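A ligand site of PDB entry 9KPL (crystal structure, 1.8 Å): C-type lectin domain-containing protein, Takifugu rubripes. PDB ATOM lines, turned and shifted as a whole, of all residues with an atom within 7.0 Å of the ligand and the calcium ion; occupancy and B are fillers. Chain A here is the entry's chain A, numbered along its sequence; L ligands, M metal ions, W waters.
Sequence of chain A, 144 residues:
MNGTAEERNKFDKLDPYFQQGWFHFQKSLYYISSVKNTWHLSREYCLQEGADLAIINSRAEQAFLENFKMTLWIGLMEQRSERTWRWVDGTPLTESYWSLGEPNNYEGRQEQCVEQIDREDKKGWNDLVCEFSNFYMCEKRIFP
Merely in contact with the ligand: Leu 128 (3.4 Å), Tyr 106 (3.6 Å) and Arg 119 (3.9 Å).
Within 4 Å of the ligand: Glu 102, Asn 104, Tyr 106, Arg 109, Glu 111, Arg 119, Lys 122, Asn 126, Asp 127 and Leu 128.
The nearest printed residue that does not touch the ligand is Phe 132 (4.8 Å).
The side-chain amino group (NZ) of Lys 122 sits at hydrogen-bond distance from an oxygen (O2) of the ligand, 3.5 Å away.
O6 of the ligand sits close to NH2 of Arg 109 (3.2 Å).
The side-chain hydroxyl (OG) of Ser 99 sits close to the side-chain amino group (NZ) of Lys 122, at 3.5 Å.
OE1 of Glu 111 lies close to N of Tyr 106 (3.0 Å).
The backbone NH (N) of Tyr 106 sits close to the side-chain amide oxygen (OD1) of Asn 104 (3.1 Å).
The side-chain carboxylate (OD2) of Asp 127 sits at hydrogen-bond distance from the backbone NH (N) of Asn 105.
OD1 of Asn 105 is in hydrogen-bond range of N of Glu 111 (2.9 Å).
The side-chain amide nitrogen (ND2) of Asn 126 sits at hydrogen-bond distance from the side-chain carboxylate (OE2) of Glu 115 (2.8 Å).
OE2 of Glu 102 lies within salt-bridge range of NZ of Lys 122, at 3.0 Å.
OD2 of Asp 127 is in salt-bridge range of NH1 of Arg 83, 3.0 Å away.
Within 4 Å of the calcium ion: Glu 102, Asn 104, Glu 111, Asn 126 and Asp 127.
The calcium ion is bound by OD1 of Asn 126, at 2.4 Å.
The side-chain carboxylate (OD1) of Asp 127 is bound to the calcium ion (2.4 Å).
The calcium ion is bound by OE1 of Glu 111 (2.4 Å).
The calcium ion is bound by OD1 of Asn 104, at 2.4 Å.
The backbone carbonyl oxygen (O) of Asp 127 is bound to the calcium ion (2.5 Å).
O3 of the ligand binds the calcium ion (2.5 Å).
The calcium ion is bound by O4 of the ligand (2.6 Å).
OE1 of Glu 102 binds the calcium ion (2.6 Å).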
ATOM      1  N   ARG A  83      11.079 -20.129 -15.996  1.00  0.00           N
ATOM      2  CA  ARG A  83      11.110 -21.551 -16.357  1.00  0.00           C
ATOM      3  C   ARG A  83      10.058 -22.297 -15.577  1.00  0.00           C
ATOM      4  O   ARG A  83      10.224 -23.474 -15.251  1.00  0.00           O
ATOM      5  CB  ARG A  83      12.484 -22.231 -16.130  1.00  0.00           C
ATOM      6  CG  ARG A  83      13.623 -21.515 -16.934  1.00  0.00           C
ATOM      7  CD  ARG A  83      13.699 -22.044 -18.363  1.00  0.00           C
ATOM      8  NE  ARG A  83      12.779 -21.430 -19.326  1.00  0.00           N
ATOM      9  CZ  ARG A  83      12.675 -21.915 -20.561  1.00  0.00           C
ATOM     10  NH1 ARG A  83      13.346 -23.018 -20.927  1.00  0.00           N
ATOM     11  NH2 ARG A  83      11.849 -21.342 -21.413  1.00  0.00           N
ATOM     12  N   SER A  99       9.048 -32.537 -25.632  1.00  0.00           N
ATOM     13  CA  SER A  99       9.894 -33.432 -26.393  1.00  0.00           C
ATOM     14  C   SER A  99      11.262 -33.524 -25.716  1.00  0.00           C
ATOM     15  O   SER A  99      11.619 -32.721 -24.845  1.00  0.00           O
ATOM     16  CB  SER A  99      10.014 -33.010 -27.864  1.00  0.00           C
ATOM     17  OG  SER A  99      10.456 -31.660 -28.036  1.00  0.00           O
ATOM     18  N   LEU A 100      12.019 -34.537 -26.081  1.00  0.00           N
ATOM     19  CA  LEU A 100      13.288 -34.789 -25.390  1.00  0.00           C
ATOM     20  C   LEU A 100      14.239 -33.578 -25.446  1.00  0.00           C
ATOM     21  O   LEU A 100      14.496 -33.019 -26.499  1.00  0.00           O
ATOM     22  CB  LEU A 100      13.940 -36.019 -26.033  1.00  0.00           C
ATOM     23  CG  LEU A 100      15.048 -36.690 -25.258  1.00  0.00           C
ATOM     24  CD1 LEU A 100      14.415 -37.839 -24.442  1.00  0.00           C
ATOM     25  CD2 LEU A 100      16.107 -37.203 -26.238  1.00  0.00           C
ATOM     26  N   GLY A 101      14.804 -33.203 -24.297  1.00  0.00           N
ATOM     27  CA  GLY A 101      15.721 -32.087 -24.325  1.00  0.00           C
ATOM     28  C   GLY A 101      15.058 -30.739 -24.087  1.00  0.00           C
ATOM     29  O   GLY A 101      15.759 -29.738 -23.865  1.00  0.00           O
ATOM     30  N   GLU A 102      13.730 -30.700 -24.011  1.00  0.00           N
ATOM     31  CA  GLU A 102      13.000 -29.424 -23.854  1.00  0.00           C
ATOM     32  C   GLU A 102      12.333 -29.366 -22.482  1.00  0.00           C
ATOM     33  O   GLU A 102      12.049 -30.398 -21.864  1.00  0.00           O
ATOM     34  CB  GLU A 102      11.908 -29.279 -24.935  1.00  0.00           C
ATOM     35  CG  GLU A 102      12.393 -29.493 -26.366  1.00  0.00           C
ATOM     36  CD  GLU A 102      13.376 -28.442 -26.841  1.00  0.00           C
ATOM     37  OE1 GLU A 102      13.447 -27.358 -26.217  1.00  0.00           O
ATOM     38  OE2 GLU A 102      14.078 -28.679 -27.876  1.00  0.00           O
ATOM     39  N   PRO A 103      12.055 -28.161 -21.986  1.00  0.00           N
ATOM     40  CA  PRO A 103      12.325 -26.836 -22.606  1.00  0.00           C
ATOM     41  C   PRO A 103      13.783 -26.433 -22.380  1.00  0.00           C
ATOM     42  O   PRO A 103      14.401 -26.902 -21.396  1.00  0.00           O
ATOM     43  CB  PRO A 103      11.329 -25.897 -21.900  1.00  0.00           C
ATOM     44  CG  PRO A 103      11.155 -26.536 -20.471  1.00  0.00           C
ATOM     45  CD  PRO A 103      11.460 -28.046 -20.636  1.00  0.00           C
ATOM     46  N   ASN A 104      14.352 -25.626 -23.277  1.00  0.00           N
ATOM     47  CA  ASN A 104      15.800 -25.442 -23.203  1.00  0.00           C
ATOM     48  C   ASN A 104      16.331 -24.038 -23.474  1.00  0.00           C
ATOM     49  O   ASN A 104      17.565 -23.887 -23.440  1.00  0.00           O
ATOM     50  CB  ASN A 104      16.491 -26.428 -24.169  1.00  0.00           C
ATOM     51  CG  ASN A 104      16.224 -26.093 -25.645  1.00  0.00           C
ATOM     52  OD1 ASN A 104      15.441 -25.204 -25.942  1.00  0.00           O
ATOM     53  ND2 ASN A 104      16.902 -26.810 -26.579  1.00  0.00           N
ATOM     54  N   ASN A 105      15.487 -23.010 -23.757  1.00  0.00           N
ATOM     55  CA  ASN A 105      16.013 -21.664 -24.073  1.00  0.00           C
ATOM     56  C   ASN A 105      17.196 -21.781 -25.039  1.00  0.00           C
ATOM     57  O   ASN A 105      18.291 -21.253 -24.787  1.00  0.00           O
ATOM     58  CB  ASN A 105      16.454 -20.899 -22.821  1.00  0.00           C
ATOM     59  CG  ASN A 105      15.283 -20.175 -22.163  1.00  0.00           C
ATOM     60  OD1 ASN A 105      14.367 -19.700 -22.859  1.00  0.00           O
ATOM     61  ND2 ASN A 105      15.298 -20.085 -20.815  1.00  0.00           N
ATOM     62  N   TYR A 106      16.963 -22.529 -26.127  1.00  0.00           N
ATOM     63  CA  TYR A 106      17.979 -22.928 -27.115  1.00  0.00           C
ATOM     64  C   TYR A 106      18.931 -21.802 -27.473  1.00  0.00           C
ATOM     65  O   TYR A 106      18.499 -20.703 -27.823  1.00  0.00           O
ATOM     66  CB  TYR A 106      17.294 -23.358 -28.401  1.00  0.00           C
ATOM     67  CG  TYR A 106      18.189 -24.097 -29.403  1.00  0.00           C
ATOM     68  CD1 TYR A 106      18.858 -25.268 -29.054  1.00  0.00           C
ATOM     69  CD2 TYR A 106      18.319 -23.612 -30.709  1.00  0.00           C
ATOM     70  CE1 TYR A 106      19.637 -25.965 -30.004  1.00  0.00           C
ATOM     71  CE2 TYR A 106      19.087 -24.327 -31.666  1.00  0.00           C
ATOM     72  CZ  TYR A 106      19.749 -25.467 -31.283  1.00  0.00           C
ATOM     73  OH  TYR A 106      20.500 -26.158 -32.187  1.00  0.00           O
ATOM     74  N   GLU A 107      20.228 -22.108 -27.440  1.00  0.00           N
ATOM     75  CA  GLU A 107      21.259 -21.149 -27.855  1.00  0.00           C
ATOM     76  C   GLU A 107      21.179 -19.845 -27.077  1.00  0.00           C
ATOM     77  O   GLU A 107      21.571 -18.785 -27.568  1.00  0.00           O
ATOM     78  CB  GLU A 107      21.168 -20.867 -29.366  1.00  0.00           C
ATOM     79  CG  GLU A 107      21.560 -22.086 -30.204  1.00  0.00           C
ATOM     80  CD  GLU A 107      21.749 -21.701 -31.648  1.00  0.00           C
ATOM     81  OE1 GLU A 107      20.798 -21.193 -32.286  1.00  0.00           O
ATOM     82  OE2 GLU A 107      22.870 -21.869 -32.148  1.00  0.00           O
ATOM     83  N   ARG A 109      18.521 -18.045 -26.315  1.00  0.00           N
ATOM     84  CA  ARG A 109      17.390 -17.209 -26.712  1.00  0.00           C
ATOM     85  C   ARG A 109      16.242 -17.348 -25.731  1.00  0.00           C
ATOM     86  O   ARG A 109      16.058 -18.398 -25.112  1.00  0.00           O
ATOM     87  CB  ARG A 109      16.844 -17.597 -28.104  1.00  0.00           C
ATOM     88  CG  ARG A 109      17.964 -17.725 -29.115  1.00  0.00           C
ATOM     89  CD  ARG A 109      17.574 -17.991 -30.547  1.00  0.00           C
ATOM     90  NE  ARG A 109      16.860 -19.254 -30.732  1.00  0.00           N
ATOM     91  CZ  ARG A 109      16.605 -19.785 -31.928  1.00  0.00           C
ATOM     92  NH1 ARG A 109      17.030 -19.217 -33.035  1.00  0.00           N
ATOM     93  NH2 ARG A 109      15.924 -20.914 -31.996  1.00  0.00           N
ATOM     94  N   GLU A 111      12.968 -18.340 -24.990  1.00  0.00           N
ATOM     95  CA  GLU A 111      11.957 -19.206 -25.604  1.00  0.00           C
ATOM     96  C   GLU A 111      10.779 -19.341 -24.653  1.00  0.00           C
ATOM     97  O   GLU A 111      10.743 -20.234 -23.834  1.00  0.00           O
ATOM     98  CB  GLU A 111      12.530 -20.549 -26.053  1.00  0.00           C
ATOM     99  CG  GLU A 111      13.715 -20.442 -27.069  1.00  0.00           C
ATOM    100  CD  GLU A 111      13.919 -21.744 -27.742  1.00  0.00           C
ATOM    101  OE1 GLU A 111      14.144 -22.727 -27.018  1.00  0.00           O
ATOM    102  OE2 GLU A 111      13.971 -21.780 -28.995  1.00  0.00           O
ATOM    103  N   GLU A 115       5.266 -24.526 -28.577  1.00  0.00           N
ATOM    104  CA  GLU A 115       4.675 -25.159 -29.752  1.00  0.00           C
ATOM    105  C   GLU A 115       4.672 -26.683 -29.605  1.00  0.00           C
ATOM    106  O   GLU A 115       5.482 -27.271 -28.876  1.00  0.00           O
ATOM    107  CB  GLU A 115       5.503 -24.779 -31.007  1.00  0.00           C
ATOM    108  CG  GLU A 115       6.932 -25.415 -30.957  1.00  0.00           C
ATOM    109  CD  GLU A 115       7.819 -25.081 -32.189  1.00  0.00           C
ATOM    110  OE1 GLU A 115       7.349 -24.368 -33.111  1.00  0.00           O
ATOM    111  OE2 GLU A 115       8.975 -25.532 -32.199  1.00  0.00           O
ATOM    112  N   ILE A 117       5.709 -29.692 -31.845  1.00  0.00           N
ATOM    113  CA  ILE A 117       6.583 -29.806 -33.007  1.00  0.00           C
ATOM    114  C   ILE A 117       6.145 -30.997 -33.837  1.00  0.00           C
ATOM    115  O   ILE A 117       5.460 -31.913 -33.379  1.00  0.00           O
ATOM    116  CB  ILE A 117       8.047 -29.933 -32.615  1.00  0.00           C
ATOM    117  CG1 ILE A 117       8.318 -31.342 -32.105  1.00  0.00           C
ATOM    118  CG2 ILE A 117       8.424 -28.874 -31.632  1.00  0.00           C
ATOM    119  CD1 ILE A 117       9.637 -31.459 -31.383  1.00  0.00           C
ATOM    120  N   ARG A 119       8.418 -33.302 -36.051  1.00  0.00           N
ATOM    121  CA  ARG A 119       9.764 -33.574 -36.521  1.00  0.00           C
ATOM    122  C   ARG A 119       9.995 -35.074 -36.563  1.00  0.00           C
ATOM    123  O   ARG A 119       9.382 -35.843 -35.811  1.00  0.00           O
ATOM    124  CB  ARG A 119      10.856 -32.905 -35.643  1.00  0.00           C
ATOM    125  CG  ARG A 119      10.908 -31.391 -35.775  1.00  0.00           C
ATOM    126  CD  ARG A 119      11.948 -30.819 -34.805  1.00  0.00           C
ATOM    127  NE  ARG A 119      13.314 -31.215 -35.131  1.00  0.00           N
ATOM    128  CZ  ARG A 119      14.181 -30.457 -35.796  1.00  0.00           C
ATOM    129  NH1 ARG A 119      13.866 -29.222 -36.159  1.00  0.00           N
ATOM    130  NH2 ARG A 119      15.382 -30.949 -36.092  1.00  0.00           N
ATOM    131  N   LYS A 122      11.436 -36.653 -33.206  1.00  0.00           N
ATOM    132  CA  LYS A 122      11.291 -35.703 -32.093  1.00  0.00           C
ATOM    133  C   LYS A 122       9.877 -35.146 -32.165  1.00  0.00           C
ATOM    134  O   LYS A 122       9.598 -34.292 -33.014  1.00  0.00           O
ATOM    135  CB  LYS A 122      12.315 -34.580 -32.186  1.00  0.00           C
ATOM    136  CG  LYS A 122      12.758 -34.050 -30.833  1.00  0.00           C
ATOM    137  CD  LYS A 122      13.610 -32.779 -30.938  1.00  0.00           C
ATOM    138  CE  LYS A 122      13.418 -31.868 -29.689  1.00  0.00           C
ATOM    139  NZ  LYS A 122      13.026 -30.433 -30.025  1.00  0.00           N
ATOM    140  N   TRP A 125       6.274 -31.196 -27.095  1.00  0.00           N
ATOM    141  CA  TRP A 125       6.302 -29.739 -27.022  1.00  0.00           C
ATOM    142  C   TRP A 125       7.737 -29.203 -27.045  1.00  0.00           C
ATOM    143  O   TRP A 125       8.697 -29.887 -26.648  1.00  0.00           O
ATOM    144  CB  TRP A 125       5.697 -29.246 -25.726  1.00  0.00           C
ATOM    145  CG  TRP A 125       4.297 -29.775 -25.401  1.00  0.00           C
ATOM    146  CD1 TRP A 125       3.374 -30.342 -26.242  1.00  0.00           C
ATOM    147  CD2 TRP A 125       3.706 -29.727 -24.099  1.00  0.00           C
ATOM    148  NE1 TRP A 125       2.187 -30.630 -25.502  1.00  0.00           N
ATOM    149  CE2 TRP A 125       2.407 -30.271 -24.191  1.00  0.00           C
ATOM    150  CE3 TRP A 125       4.151 -29.238 -22.860  1.00  0.00           C
ATOM    151  CZ2 TRP A 125       1.569 -30.340 -23.092  1.00  0.00           C
ATOM    152  CZ3 TRP A 125       3.341 -29.354 -21.758  1.00  0.00           C
ATOM    153  CH2 TRP A 125       2.070 -29.911 -21.877  1.00  0.00           C
ATOM    154  N   ASN A 126       7.844 -27.935 -27.436  1.00  0.00           N
ATOM    155  CA  ASN A 126       9.141 -27.266 -27.553  1.00  0.00           C
ATOM    156  C   ASN A 126       8.914 -25.818 -27.134  1.00  0.00           C
ATOM    157  O   ASN A 126       7.898 -25.210 -27.549  1.00  0.00           O
ATOM    158  CB  ASN A 126       9.705 -27.332 -28.991  1.00  0.00           C
ATOM    159  CG  ASN A 126      10.915 -26.411 -29.156  1.00  0.00           C
ATOM    160  OD1 ASN A 126      11.860 -26.476 -28.330  1.00  0.00           O
ATOM    161  ND2 ASN A 126      10.917 -25.572 -30.211  1.00  0.00           N
ATOM    162  N   ASP A 127       9.776 -25.290 -26.264  1.00  0.00           N
ATOM    163  CA  ASP A 127       9.730 -23.849 -26.056  1.00  0.00           C
ATOM    164  C   ASP A 127      10.401 -23.121 -27.234  1.00  0.00           C
ATOM    165  O   ASP A 127      11.445 -23.566 -27.756  1.00  0.00           O
ATOM    166  CB  ASP A 127      10.356 -23.428 -24.708  1.00  0.00           C
ATOM    167  CG  ASP A 127      11.853 -23.842 -24.549  1.00  0.00           C
ATOM    168  OD1 ASP A 127      12.288 -24.850 -25.164  1.00  0.00           O
ATOM    169  OD2 ASP A 127      12.558 -23.192 -23.767  1.00  0.00           O
ATOM    170  N   LEU A 128       9.764 -22.027 -27.669  1.00  0.00           N
ATOM    171  CA  LEU A 128      10.209 -21.251 -28.844  1.00  0.00           C
ATOM    172  C   LEU A 128      10.036 -19.755 -28.612  1.00  0.00           C
ATOM    173  O   LEU A 128       9.215 -19.313 -27.827  1.00  0.00           O
ATOM    174  CB  LEU A 128       9.367 -21.664 -30.088  1.00  0.00           C
ATOM    175  CG  LEU A 128       9.943 -21.248 -31.442  1.00  0.00           C
ATOM    176  CD1 LEU A 128      11.228 -21.980 -31.556  1.00  0.00           C
ATOM    177  CD2 LEU A 128       8.959 -21.591 -32.591  1.00  0.00           C
ATOM    178  N   VAL A 129      10.864 -18.949 -29.310  1.00  0.00           N
ATOM    179  CA  VAL A 129      10.680 -17.482 -29.304  1.00  0.00           C
ATOM    180  C   VAL A 129       9.230 -17.125 -29.680  1.00  0.00           C
ATOM    181  O   VAL A 129       8.686 -17.585 -30.702  1.00  0.00           O
ATOM    182  CB  VAL A 129      11.657 -16.847 -30.278  1.00  0.00           C
ATOM    183  CG1 VAL A 129      11.465 -15.359 -30.242  1.00  0.00           C
ATOM    184  CG2 VAL A 129      13.076 -17.232 -29.880  1.00  0.00           C
ATOM    185  N   PHE A 132       8.416 -15.803 -33.270  1.00  0.00           N
ATOM    186  CA  PHE A 132       8.443 -16.667 -34.443  1.00  0.00           C
ATOM    187  C   PHE A 132       7.009 -17.046 -34.843  1.00  0.00           C
ATOM    188  O   PHE A 132       6.081 -16.874 -34.066  1.00  0.00           O
ATOM    189  CB  PHE A 132       9.221 -17.964 -34.179  1.00  0.00           C
ATOM    190  CG  PHE A 132      10.725 -17.764 -33.992  1.00  0.00           C
ATOM    191  CD1 PHE A 132      11.282 -16.482 -33.989  1.00  0.00           C
ATOM    192  CD2 PHE A 132      11.580 -18.876 -33.827  1.00  0.00           C
ATOM    193  CE1 PHE A 132      12.684 -16.312 -33.790  1.00  0.00           C
ATOM    194  CE2 PHE A 132      12.991 -18.716 -33.632  1.00  0.00           C
ATOM    195  CZ  PHE A 132      13.529 -17.430 -33.606  1.00  0.00           C
HETATM  196  C1  LIG L   1      15.853 -26.572 -32.425  1.00  0.00           C
HETATM  197  C2  LIG L   1      15.920 -26.952 -30.877  1.00  0.00           C
HETATM  198  C3  LIG L   1      14.721 -26.291 -30.083  1.00  0.00           C
HETATM  199  C4  LIG L   1      14.695 -24.747 -30.437  1.00  0.00           C
HETATM  200  C5  LIG L   1      14.480 -24.669 -31.984  1.00  0.00           C
HETATM  201  C6  LIG L   1      14.253 -23.260 -32.420  1.00  0.00           C
HETATM  202  O1  LIG L   1      14.758 -27.252 -32.920  1.00  0.00           O
HETATM  203  O2  LIG L   1      15.733 -28.344 -30.759  1.00  0.00           O
HETATM  204  O3  LIG L   1      14.965 -26.415 -28.727  1.00  0.00           O
HETATM  205  O4  LIG L   1      13.654 -24.110 -29.667  1.00  0.00           O
HETATM  206  O5  LIG L   1      15.572 -25.197 -32.658  1.00  0.00           O
HETATM  207  O6  LIG L   1      14.574 -23.236 -33.795  1.00  0.00           O
HETATM  208 CA    CA M   1      13.406 -25.021 -27.290  1.00  0.00          CA
HETATM  209  O   HOH W   1      12.534 -23.016 -35.074  1.00  0.00           O
